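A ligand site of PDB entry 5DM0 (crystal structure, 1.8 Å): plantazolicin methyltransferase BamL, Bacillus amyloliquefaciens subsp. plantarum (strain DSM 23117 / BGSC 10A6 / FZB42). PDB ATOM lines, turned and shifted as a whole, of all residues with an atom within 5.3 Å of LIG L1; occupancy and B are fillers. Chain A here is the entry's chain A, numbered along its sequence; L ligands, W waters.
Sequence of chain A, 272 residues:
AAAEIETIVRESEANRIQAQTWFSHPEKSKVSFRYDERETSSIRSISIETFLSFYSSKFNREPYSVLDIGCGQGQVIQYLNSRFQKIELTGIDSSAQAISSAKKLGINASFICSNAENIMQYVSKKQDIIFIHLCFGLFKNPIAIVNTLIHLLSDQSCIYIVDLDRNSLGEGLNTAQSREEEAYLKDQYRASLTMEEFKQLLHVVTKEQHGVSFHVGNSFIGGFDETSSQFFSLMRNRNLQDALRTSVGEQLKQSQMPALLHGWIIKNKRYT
A nitrogen (N4) of LIG L1 lies within hydrogen-bond range of the backbone carbonyl oxygen of Leu 134, 2.9 Å away. A nitrogen (N6) of LIG L1 lies within salt-bridge range of the side-chain carboxylate of Asp 163. N6 of LIG L1 lies within hydrogen-bond range of OG of Ser 192. N7 of LIG L1 lies within hydrogen-bond range of O of Gln 188 (3.0 Å). NE2 of Gln 188 lies close to N7 of LIG L1 (3.0 Å). A sulfur (S2) of LIG L1 sits close to the side-chain hydroxyl of Tyr 184 (3.1 Å). The side-chain hydroxyl of Tyr 35 sits close to a sulfur (S1) of LIG L1, at 3.4 Å. The side-chain carboxylate (OD2) of Asp 36 lies within salt-bridge range of a nitrogen (N4) of LIG L1 (3.6 Å).
N4 of LIG L1 sits close to S1 of LG2 L2, at 3.4 Å.
The side-chain carboxylate (OD2) of Asp 163 is in hydrogen-bond range of the backbone NH (N) of Gly 137 (3.0 Å). O of Gln 188 lies within hydrogen-bond range of OG of Ser 192 (2.8 Å). OG of Ser 192 sits close to O of Tyr 189 (3.4 Å). The side-chain amide oxygen (OE1) of Gln 188 lies close to the backbone carbonyl oxygen (O) of Ala 19 (3.0 Å). OH of Tyr 184 sits at hydrogen-bond distance from OD1 of Asp 36 (2.7 Å). The backbone carbonyl oxygen of Asp 36 lies within hydrogen-bond range of the side-chain hydroxyl of Thr 40 (2.6 Å). The side-chain hydroxyl (OH) of Tyr 35 is in hydrogen-bond range of the side-chain hydroxyl (OG1) of Thr 175, 2.6 Å away.
An oxygen (O1) of LIG L1 lies close to the side-chain sulfur of Met 257, 3.3 Å away. Phe 23 touches LIG L1. Thr 40 touches LIG L1. Ile 43 touches LIG L1 (CG2 to C11, 3.9 Å). Cys 135 touches LIG L1. CA of Gly 137 touches N6 of LIG L1, at 3.6 Å. CG of Leu 138 touches C15 of LIG L1, at 3.6 Å. CD2 of Leu 164 touches C6 of LIG L1, at 3.6 Å. Leu 185 touches LIG L1. CE1 of Phe 220 touches C17 of LIG L1, at 3.97 Å. OE1 of Gln 251 touches C18 of LIG L1, 3.9 Å away. CG of Pro 258 touches C8 of LIG L1, 3.7 Å away. Leu 260 touches LIG L1. Within 4 Å of LIG L1: Phe 23, Tyr 35, Asp 36, Thr 40, Ile 43, Leu 134, Cys 135, Gly 137, Leu 138, Asp 163, Leu 164, Tyr 184, Leu 185, Gln 188, Ser 192, Phe 220, Gln 251, Met 257, Pro 258 and Leu 260.
Water W1 lies within hydrogen-bond range of a nitrogen (N4) of LIG L1 (2.8 Å), the side-chain hydroxyl of Thr 40 (2.8 Å) and an oxygen (O1) of LG2 L2 (2.9 Å). Water W2 lies within hydrogen-bond range of OH of Tyr 189, OH of Tyr 35 and N2 of LIG L1.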
ATOM      1  N   ALA A  19      12.338   0.644  20.687  1.00  0.00           N
ATOM      2  CA  ALA A  19      13.198   0.697  19.500  1.00  0.00           C
ATOM      3  C   ALA A  19      14.631   0.311  19.853  1.00  0.00           C
ATOM      4  O   ALA A  19      15.303  -0.375  19.087  1.00  0.00           O
ATOM      5  CB  ALA A  19      13.164   2.086  18.862  1.00  0.00           C
ATOM      6  N   PHE A  23      18.935  -2.986  19.483  1.00  0.00           N
ATOM      7  CA  PHE A  23      20.385  -2.812  19.533  1.00  0.00           C
ATOM      8  C   PHE A  23      20.997  -3.385  20.808  1.00  0.00           C
ATOM      9  O   PHE A  23      22.210  -3.480  20.914  1.00  0.00           O
ATOM     10  CB  PHE A  23      20.733  -1.335  19.357  1.00  0.00           C
ATOM     11  CG  PHE A  23      20.340  -0.822  18.003  1.00  0.00           C
ATOM     12  CD1 PHE A  23      21.160  -1.057  16.907  1.00  0.00           C
ATOM     13  CD2 PHE A  23      19.109  -0.203  17.820  1.00  0.00           C
ATOM     14  CE1 PHE A  23      20.774  -0.639  15.637  1.00  0.00           C
ATOM     15  CE2 PHE A  23      18.708   0.209  16.556  1.00  0.00           C
ATOM     16  CZ  PHE A  23      19.546  -0.015  15.466  1.00  0.00           C
ATOM     17  N   TYR A  35      20.033  -5.251   8.466  1.00  0.00           N
ATOM     18  CA  TYR A  35      19.265  -4.235   7.745  1.00  0.00           C
ATOM     19  C   TYR A  35      20.075  -2.953   7.537  1.00  0.00           C
ATOM     20  O   TYR A  35      20.187  -2.453   6.408  1.00  0.00           O
ATOM     21  CB  TYR A  35      17.938  -3.939   8.443  1.00  0.00           C
ATOM     22  CG  TYR A  35      17.167  -2.850   7.727  1.00  0.00           C
ATOM     23  CD1 TYR A  35      17.432  -1.501   7.999  1.00  0.00           C
ATOM     24  CD2 TYR A  35      16.209  -3.160   6.762  1.00  0.00           C
ATOM     25  CE1 TYR A  35      16.758  -0.493   7.340  1.00  0.00           C
ATOM     26  CE2 TYR A  35      15.513  -2.150   6.099  1.00  0.00           C
ATOM     27  CZ  TYR A  35      15.803  -0.828   6.394  1.00  0.00           C
ATOM     28  OH  TYR A  35      15.140   0.188   5.753  1.00  0.00           O
ATOM     29  N   ASP A  36      20.627  -2.412   8.624  1.00  0.00           N
ATOM     30  CA  ASP A  36      21.377  -1.144   8.565  1.00  0.00           C
ATOM     31  C   ASP A  36      22.521  -1.180   7.554  1.00  0.00           C
ATOM     32  O   ASP A  36      22.680  -0.266   6.753  1.00  0.00           O
ATOM     33  CB  ASP A  36      21.882  -0.764   9.963  1.00  0.00           C
ATOM     34  CG  ASP A  36      20.754  -0.473  10.944  1.00  0.00           C
ATOM     35  OD1 ASP A  36      19.570  -0.510  10.550  1.00  0.00           O
ATOM     36  OD2 ASP A  36      21.050  -0.216  12.137  1.00  0.00           O
ATOM     37  N   GLU A  39      20.868  -1.321   3.869  1.00  0.00           N
ATOM     38  CA  GLU A  39      19.997  -0.226   3.414  1.00  0.00           C
ATOM     39  C   GLU A  39      20.413   1.202   3.805  1.00  0.00           C
ATOM     40  O   GLU A  39      19.911   2.161   3.225  1.00  0.00           O
ATOM     41  CB  GLU A  39      18.552  -0.473   3.885  1.00  0.00           C
ATOM     42  CG  GLU A  39      17.948  -1.798   3.425  1.00  0.00           C
ATOM     43  CD  GLU A  39      17.660  -1.856   1.935  1.00  0.00           C
ATOM     44  OE1 GLU A  39      17.610  -0.790   1.287  1.00  0.00           O
ATOM     45  OE2 GLU A  39      17.473  -2.979   1.401  1.00  0.00           O
ATOM     46  N   THR A  40      21.306   1.335   4.782  1.00  0.00           N
ATOM     47  CA  THR A  40      21.668   2.666   5.296  1.00  0.00           C
ATOM     48  C   THR A  40      23.121   3.097   5.007  1.00  0.00           C
ATOM     49  O   THR A  40      23.513   4.227   5.322  1.00  0.00           O
ATOM     50  CB  THR A  40      21.326   2.839   6.799  1.00  0.00           C
ATOM     51  OG1 THR A  40      22.320   2.190   7.604  1.00  0.00           O
ATOM     52  CG2 THR A  40      19.957   2.233   7.111  1.00  0.00           C
ATOM     53  N   SER A  42      24.607   3.521   2.017  1.00  0.00           N
ATOM     54  CA  SER A  42      24.705   4.437   0.869  1.00  0.00           C
ATOM     55  C   SER A  42      24.647   5.918   1.233  1.00  0.00           C
ATOM     56  O   SER A  42      25.356   6.736   0.646  1.00  0.00           O
ATOM     57  CB  SER A  42      23.601   4.127  -0.150  1.00  0.00           C
ATOM     58  OG  SER A  42      23.789   2.843  -0.703  1.00  0.00           O
ATOM     59  N   ILE A  43      23.808   6.253   2.206  1.00  0.00           N
ATOM     60  CA  ILE A  43      23.622   7.637   2.623  1.00  0.00           C
ATOM     61  C   ILE A  43      24.807   8.196   3.425  1.00  0.00           C
ATOM     62  O   ILE A  43      24.980   9.403   3.522  1.00  0.00           O
ATOM     63  CB  ILE A  43      22.328   7.796   3.466  1.00  0.00           C
ATOM     64  CG1 ILE A  43      21.798   9.221   3.351  1.00  0.00           C
ATOM     65  CG2 ILE A  43      22.579   7.424   4.929  1.00  0.00           C
ATOM     66  CD1 ILE A  43      20.452   9.410   3.992  1.00  0.00           C
ATOM     67  N   LEU A 134      21.270   8.681  12.329  1.00  0.00           N
ATOM     68  CA  LEU A 134      20.349   7.554  12.377  1.00  0.00           C
ATOM     69  C   LEU A 134      20.265   6.854  13.747  1.00  0.00           C
ATOM     70  O   LEU A 134      20.198   5.618  13.807  1.00  0.00           O
ATOM     71  CB  LEU A 134      20.671   6.537  11.265  1.00  0.00           C
ATOM     72  CG  LEU A 134      20.896   7.139   9.869  1.00  0.00           C
ATOM     73  CD1 LEU A 134      21.355   6.086   8.871  1.00  0.00           C
ATOM     74  CD2 LEU A 134      19.630   7.839   9.391  1.00  0.00           C
ATOM     75  N   CYS A 135      20.242   7.648  14.823  1.00  0.00           N
ATOM     76  CA  CYS A 135      20.118   7.088  16.183  1.00  0.00           C
ATOM     77  C   CYS A 135      19.322   7.926  17.195  1.00  0.00           C
ATOM     78  O   CYS A 135      19.091   7.483  18.324  1.00  0.00           O
ATOM     79  CB  CYS A 135      21.497   6.736  16.757  1.00  0.00           C
ATOM     80  SG  CYS A 135      22.604   8.151  17.001  1.00  0.00           S
ATOM     81  N   PHE A 136      18.885   9.124  16.790  1.00  0.00           N
ATOM     82  CA  PHE A 136      18.266  10.062  17.728  1.00  0.00           C
ATOM     83  C   PHE A 136      17.071   9.454  18.473  1.00  0.00           C
ATOM     84  O   PHE A 136      16.930   9.623  19.690  1.00  0.00           O
ATOM     85  CB  PHE A 136      17.873  11.347  17.000  1.00  0.00           C
ATOM     86  CG  PHE A 136      17.571  12.513  17.899  1.00  0.00           C
ATOM     87  CD1 PHE A 136      18.531  12.987  18.786  1.00  0.00           C
ATOM     88  CD2 PHE A 136      16.331  13.160  17.833  1.00  0.00           C
ATOM     89  CE1 PHE A 136      18.253  14.077  19.613  1.00  0.00           C
ATOM     90  CE2 PHE A 136      16.059  14.242  18.669  1.00  0.00           C
ATOM     91  CZ  PHE A 136      17.025  14.711  19.549  1.00  0.00           C
ATOM     92  N   GLY A 137      16.232   8.726  17.735  1.00  0.00           N
ATOM     93  CA  GLY A 137      15.009   8.152  18.294  1.00  0.00           C
ATOM     94  C   GLY A 137      15.268   6.973  19.220  1.00  0.00           C
ATOM     95  O   GLY A 137      14.335   6.392  19.763  1.00  0.00           O
ATOM     96  N   LEU A 138      16.541   6.611  19.407  1.00  0.00           N
ATOM     97  CA  LEU A 138      16.893   5.528  20.354  1.00  0.00           C
ATOM     98  C   LEU A 138      17.163   6.051  21.763  1.00  0.00           C
ATOM     99  O   LEU A 138      17.186   5.291  22.728  1.00  0.00           O
ATOM    100  CB  LEU A 138      18.089   4.737  19.843  1.00  0.00           C
ATOM    101  CG  LEU A 138      17.940   4.071  18.466  1.00  0.00           C
ATOM    102  CD1 LEU A 138      19.265   3.452  18.067  1.00  0.00           C
ATOM    103  CD2 LEU A 138      16.811   3.046  18.457  1.00  0.00           C
ATOM    104  N   ASP A 163      17.795  11.619  10.996  1.00  0.00           N
ATOM    105  CA  ASP A 163      17.018  10.513  11.553  1.00  0.00           C
ATOM    106  C   ASP A 163      15.732  10.272  10.775  1.00  0.00           C
ATOM    107  O   ASP A 163      15.338  11.080   9.922  1.00  0.00           O
ATOM    108  CB  ASP A 163      16.715  10.760  13.035  1.00  0.00           C
ATOM    109  CG  ASP A 163      16.535   9.469  13.828  1.00  0.00           C
ATOM    110  OD1 ASP A 163      17.009   8.413  13.356  1.00  0.00           O
ATOM    111  OD2 ASP A 163      15.889   9.502  14.908  1.00  0.00           O
ATOM    112  N   LEU A 164      15.080   9.147  11.055  1.00  0.00           N
ATOM    113  CA  LEU A 164      13.825   8.783  10.425  1.00  0.00           C
ATOM    114  C   LEU A 164      12.726   9.771  10.780  1.00  0.00           C
ATOM    115  O   LEU A 164      12.688  10.286  11.888  1.00  0.00           O
ATOM    116  CB  LEU A 164      13.384   7.409  10.919  1.00  0.00           C
ATOM    117  CG  LEU A 164      14.366   6.251  10.745  1.00  0.00           C
ATOM    118  CD1 LEU A 164      13.730   4.993  11.325  1.00  0.00           C
ATOM    119  CD2 LEU A 164      14.692   6.092   9.264  1.00  0.00           C
ATOM    120  N   THR A 175      11.532  -1.526   1.937  1.00  0.00           N
ATOM    121  CA  THR A 175      12.926  -1.978   1.906  1.00  0.00           C
ATOM    122  C   THR A 175      13.176  -3.223   2.769  1.00  0.00           C
ATOM    123  O   THR A 175      14.260  -3.807   2.746  1.00  0.00           O
ATOM    124  CB  THR A 175      13.901  -0.871   2.368  1.00  0.00           C
ATOM    125  OG1 THR A 175      13.646  -0.554   3.741  1.00  0.00           O
ATOM    126  CG2 THR A 175      13.769   0.376   1.508  1.00  0.00           C
ATOM    127  N   TYR A 184      11.153  -4.793  13.044  1.00  0.00           N
ATOM    128  CA  TYR A 184      12.235  -3.881  13.389  1.00  0.00           C
ATOM    129  C   TYR A 184      11.846  -2.462  12.988  1.00  0.00           C
ATOM    130  O   TYR A 184      11.840  -1.553  13.829  1.00  0.00           O
ATOM    131  CB  TYR A 184      13.508  -4.320  12.660  1.00  0.00           C
ATOM    132  CG  TYR A 184      14.647  -3.332  12.644  1.00  0.00           C
ATOM    133  CD1 TYR A 184      15.155  -2.786  13.834  1.00  0.00           C
ATOM    134  CD2 TYR A 184      15.266  -2.978  11.443  1.00  0.00           C
ATOM    135  CE1 TYR A 184      16.218  -1.892  13.809  1.00  0.00           C
ATOM    136  CE2 TYR A 184      16.334  -2.089  11.410  1.00  0.00           C
ATOM    137  CZ  TYR A 184      16.808  -1.559  12.600  1.00  0.00           C
ATOM    138  OH  TYR A 184      17.856  -0.671  12.580  1.00  0.00           O
ATOM    139  N   LEU A 185      11.482  -2.285  11.724  1.00  0.00           N
ATOM    140  CA  LEU A 185      11.134  -0.944  11.206  1.00  0.00           C
ATOM    141  C   LEU A 185       9.881  -0.378  11.837  1.00  0.00           C
ATOM    142  O   LEU A 185       9.817   0.817  12.132  1.00  0.00           O
ATOM    143  CB  LEU A 185      11.036  -0.957   9.675  1.00  0.00           C
ATOM    144  CG  LEU A 185      12.323  -1.298   8.920  1.00  0.00           C
ATOM    145  CD1 LEU A 185      12.064  -1.323   7.415  1.00  0.00           C
ATOM    146  CD2 LEU A 185      13.477  -0.346   9.237  1.00  0.00           C
ATOM    147  N   GLN A 188      11.131   1.023  14.960  1.00  0.00           N
ATOM    148  CA  GLN A 188      12.018   2.180  14.738  1.00  0.00           C
ATOM    149  C   GLN A 188      11.217   3.409  14.348  1.00  0.00           C
ATOM    150  O   GLN A 188      11.432   4.494  14.885  1.00  0.00           O
ATOM    151  CB  GLN A 188      13.044   1.879  13.657  1.00  0.00           C
ATOM    152  CG  GLN A 188      13.996   0.725  13.985  1.00  0.00           C
ATOM    153  CD  GLN A 188      14.653   0.847  15.358  1.00  0.00           C
ATOM    154  OE1 GLN A 188      14.628  -0.090  16.163  1.00  0.00           O
ATOM    155  NE2 GLN A 188      15.227   2.018  15.643  1.00  0.00           N
ATOM    156  N   TYR A 189      10.287   3.258  13.412  1.00  0.00           N
ATOM    157  CA  TYR A 189       9.511   4.408  12.965  1.00  0.00           C
ATOM    158  C   TYR A 189       8.582   4.909  14.072  1.00  0.00           C
ATOM    159  O   TYR A 189       8.414   6.131  14.226  1.00  0.00           O
ATOM    160  CB  TYR A 189       8.766   4.108  11.657  1.00  0.00           C
ATOM    161  CG  TYR A 189       9.663   4.207  10.440  1.00  0.00           C
ATOM    162  CD1 TYR A 189       9.849   5.430   9.782  1.00  0.00           C
ATOM    163  CD2 TYR A 189      10.330   3.081   9.948  1.00  0.00           C
ATOM    164  CE1 TYR A 189      10.670   5.524   8.681  1.00  0.00           C
ATOM    165  CE2 TYR A 189      11.163   3.163   8.850  1.00  0.00           C
ATOM    166  CZ  TYR A 189      11.331   4.391   8.218  1.00  0.00           C
ATOM    167  OH  TYR A 189      12.143   4.502   7.126  1.00  0.00           O
ATOM    168  N   ALA A 191       9.160   5.002  17.183  1.00  0.00           N
ATOM    169  CA  ALA A 191       9.984   5.757  18.120  1.00  0.00           C
ATOM    170  C   ALA A 191      10.497   7.076  17.547  1.00  0.00           C
ATOM    171  O   ALA A 191      11.043   7.895  18.287  1.00  0.00           O
ATOM    172  CB  ALA A 191      11.172   4.907  18.568  1.00  0.00           C
ATOM    173  N   SER A 192      10.329   7.291  16.252  1.00  0.00           N
ATOM    174  CA  SER A 192      10.859   8.482  15.592  1.00  0.00           C
ATOM    175  C   SER A 192      10.002   9.718  15.852  1.00  0.00           C
ATOM    176  O   SER A 192       8.833   9.612  16.255  1.00  0.00           O
ATOM    177  CB  SER A 192      10.999   8.240  14.082  1.00  0.00           C
ATOM    178  OG  SER A 192      11.698   7.041  13.834  1.00  0.00           O
ATOM    179  N   PHE A 220      16.649  16.234   0.603  1.00  0.00           N
ATOM    180  CA  PHE A 220      17.687  15.219   0.548  1.00  0.00           C
ATOM    181  C   PHE A 220      19.055  15.684   1.040  1.00  0.00           C
ATOM    182  O   PHE A 220      19.773  14.913   1.688  1.00  0.00           O
ATOM    183  CB  PHE A 220      17.799  14.680  -0.886  1.00  0.00           C
ATOM    184  CG  PHE A 220      18.705  13.493  -1.012  1.00  0.00           C
ATOM    185  CD1 PHE A 220      18.462  12.330  -0.281  1.00  0.00           C
ATOM    186  CD2 PHE A 220      19.802  13.521  -1.874  1.00  0.00           C
ATOM    187  CE1 PHE A 220      19.294  11.227  -0.406  1.00  0.00           C
ATOM    188  CE2 PHE A 220      20.635  12.426  -2.004  1.00  0.00           C
ATOM    189  CZ  PHE A 220      20.380  11.276  -1.276  1.00  0.00           C
ATOM    190  N   GLN A 251      19.309   4.228  -5.824  1.00  0.00           N
ATOM    191  CA  GLN A 251      18.038   4.757  -5.339  1.00  0.00           C
ATOM    192  C   GLN A 251      16.903   4.799  -6.374  1.00  0.00           C
ATOM    193  O   GLN A 251      17.136   4.906  -7.577  1.00  0.00           O
ATOM    194  CB  GLN A 251      18.243   6.131  -4.689  1.00  0.00           C
ATOM    195  CG  GLN A 251      18.994   7.149  -5.533  1.00  0.00           C
ATOM    196  CD  GLN A 251      19.460   8.350  -4.726  1.00  0.00           C
ATOM    197  OE1 GLN A 251      18.960   8.606  -3.626  1.00  0.00           O
ATOM    198  NE2 GLN A 251      20.426   9.088  -5.263  1.00  0.00           N
ATOM    199  N   MET A 257      11.108   6.650  -1.596  1.00  0.00           N
ATOM    200  CA  MET A 257      12.107   6.460  -0.522  1.00  0.00           C
ATOM    201  C   MET A 257      11.683   7.192   0.773  1.00  0.00           C
ATOM    202  O   MET A 257      11.011   8.205   0.695  1.00  0.00           O
ATOM    203  CB  MET A 257      13.485   6.931  -0.981  1.00  0.00           C
ATOM    204  CG  MET A 257      13.749   6.734  -2.470  1.00  0.00           C
ATOM    205  SD  MET A 257      15.399   6.122  -2.867  1.00  0.00           S
ATOM    206  CE  MET A 257      15.178   4.350  -2.596  1.00  0.00           C
ATOM    207  N   PRO A 258      12.074   6.658   1.953  1.00  0.00           N
ATOM    208  CA  PRO A 258      11.677   7.305   3.226  1.00  0.00           C
ATOM    209  C   PRO A 258      12.306   8.679   3.417  1.00  0.00           C
ATOM    210  O   PRO A 258      13.515   8.831   3.270  1.00  0.00           O
ATOM    211  CB  PRO A 258      12.195   6.334   4.296  1.00  0.00           C
ATOM    212  CG  PRO A 258      13.263   5.547   3.613  1.00  0.00           C
ATOM    213  CD  PRO A 258      12.808   5.408   2.193  1.00  0.00           C
ATOM    214  N   LEU A 260      13.833  11.705   5.413  1.00  0.00           N
ATOM    215  CA  LEU A 260      14.588  11.841   6.652  1.00  0.00           C
ATOM    216  C   LEU A 260      14.506  13.237   7.239  1.00  0.00           C
ATOM    217  O   LEU A 260      14.380  14.217   6.506  1.00  0.00           O
ATOM    218  CB  LEU A 260      16.064  11.474   6.443  1.00  0.00           C
ATOM    219  CG  LEU A 260      16.325  10.067   5.899  1.00  0.00           C
ATOM    220  CD1 LEU A 260      17.792   9.973   5.530  1.00  0.00           C
ATOM    221  CD2 LEU A 260      15.958   8.963   6.895  1.00  0.00           C
HETATM  222  C1  LIG L   1      16.103   2.266   9.501  1.00  0.00           C
HETATM  223  C2  LIG L   1      17.145   3.170   9.267  1.00  0.00           C
HETATM  224  C3  LIG L   1      17.113   4.377   5.977  1.00  0.00           C
HETATM  225  C4  LIG L   1      17.981   2.561  11.235  1.00  0.00           C
HETATM  226  C5  LIG L   1      18.129   5.274   6.553  1.00  0.00           C
HETATM  227  C6  LIG L   1      17.298   3.902   7.985  1.00  0.00           C
HETATM  228  C7  LIG L   1      16.766   4.312   4.560  1.00  0.00           C
HETATM  229  C8  LIG L   1      16.084   3.617   2.297  1.00  0.00           C
HETATM  230  C9  LIG L   1      16.803   4.811   2.393  1.00  0.00           C
HETATM  231  O1  LIG L   1      16.497   5.457   0.163  1.00  0.00           O
HETATM  232  C10 LIG L   1      17.132   5.621   1.193  1.00  0.00           C
HETATM  233  O2  LIG L   1      18.241   6.560   1.271  1.00  0.00           O
HETATM  234  N1  LIG L   1      17.209   5.182   3.650  1.00  0.00           N
HETATM  235  S1  LIG L   1      15.930   2.976   3.887  1.00  0.00           S
HETATM  236  N2  LIG L   1      16.663   3.486   6.867  1.00  0.00           N
HETATM  237  O3  LIG L   1      18.211   4.932   7.881  1.00  0.00           O
HETATM  238  C11 LIG L   1      18.963   6.428   6.065  1.00  0.00           C
HETATM  239  S2  LIG L   1      16.508   1.643  11.064  1.00  0.00           S
HETATM  240  N3  LIG L   1      18.176   3.315  10.141  1.00  0.00           N
HETATM  241  C12 LIG L   1      18.811   2.414  12.463  1.00  0.00           C
HETATM  242  N4  LIG L   1      20.030   3.197  12.302  1.00  0.00           N
HETATM  243  C13 LIG L   1      18.066   2.839  13.732  1.00  0.00           C
HETATM  244  C14 LIG L   1      17.346   4.183  13.612  1.00  0.00           C
HETATM  245  C15 LIG L   1      17.174   4.755  15.021  1.00  0.00           C
HETATM  246  N5  LIG L   1      16.288   5.922  14.920  1.00  0.00           N
HETATM  247  C16 LIG L   1      15.021   5.942  15.022  1.00  0.00           C
HETATM  248  N6  LIG L   1      14.387   7.041  14.903  1.00  0.00           N
HETATM  249  N7  LIG L   1      14.360   4.872  15.230  1.00  0.00           N
HETATM  250  C17 LIG L   1      18.597   7.358   0.144  1.00  0.00           C
HETATM  251  C18 LIG L   1      20.060   7.145  -0.193  1.00  0.00           C
HETATM  252  N1  LG2 L   2      25.487   6.262  13.570  1.00  0.00           N
HETATM  253  C1  LG2 L   2      25.147   4.898  13.066  1.00  0.00           C
HETATM  254  C2  LG2 L   2      23.860   4.408  13.720  1.00  0.00           C
HETATM  255  C3  LG2 L   2      23.968   2.895  13.928  1.00  0.00           C
HETATM  256  S1  LG2 L   2      22.466   2.186  14.521  1.00  0.00           S
HETATM  257  C4  LG2 L   2      24.973   4.976  11.573  1.00  0.00           C
HETATM  258  O1  LG2 L   2      24.426   4.080  10.926  1.00  0.00           O
HETATM  259  O2  LG2 L   2      25.406   5.940  10.948  1.00  0.00           O
HETATM  260  C5  LG2 L   2      22.187   3.043  16.042  1.00  0.00           C
HETATM  261  C6  LG2 L   2      23.380   2.980  16.994  1.00  0.00           C
HETATM  262  O3  LG2 L   2      23.098   3.785  18.150  1.00  0.00           O
HETATM  263  C7  LG2 L   2      23.663   1.573  17.535  1.00  0.00           C
HETATM  264  O4  LG2 L   2      25.037   1.232  17.272  1.00  0.00           O
HETATM  265  C8  LG2 L   2      23.399   1.649  19.033  1.00  0.00           C
HETATM  266  O5  LG2 L   2      24.272   0.823  19.807  1.00  0.00           O
HETATM  267  C9  LG2 L   2      23.632   3.130  19.306  1.00  0.00           C
HETATM  268  N2  LG2 L   2      22.965   3.673  20.500  1.00  0.00           N
HETATM  269  C10 LG2 L   2      21.681   3.496  20.876  1.00  0.00           C
HETATM  270  N3  LG2 L   2      21.426   4.184  22.017  1.00  0.00           N
HETATM  271  C11 LG2 L   2      22.566   4.796  22.379  1.00  0.00           C
HETATM  272  C12 LG2 L   2      23.002   5.680  23.489  1.00  0.00           C
HETATM  273  N4  LG2 L   2      22.142   6.045  24.468  1.00  0.00           N
HETATM  274  N5  LG2 L   2      24.291   6.090  23.473  1.00  0.00           N
HETATM  275  C13 LG2 L   2      25.170   5.734  22.517  1.00  0.00           C
HETATM  276  N6  LG2 L   2      24.846   4.943  21.472  1.00  0.00           N
HETATM  277  C14 LG2 L   2      23.576   4.456  21.369  1.00  0.00           C
HETATM  278  O   HOH W   1      21.889   2.740  10.325  1.00  0.00           O
HETATM  279  O   HOH W   2      13.942   2.511   6.878  1.00  0.00           O
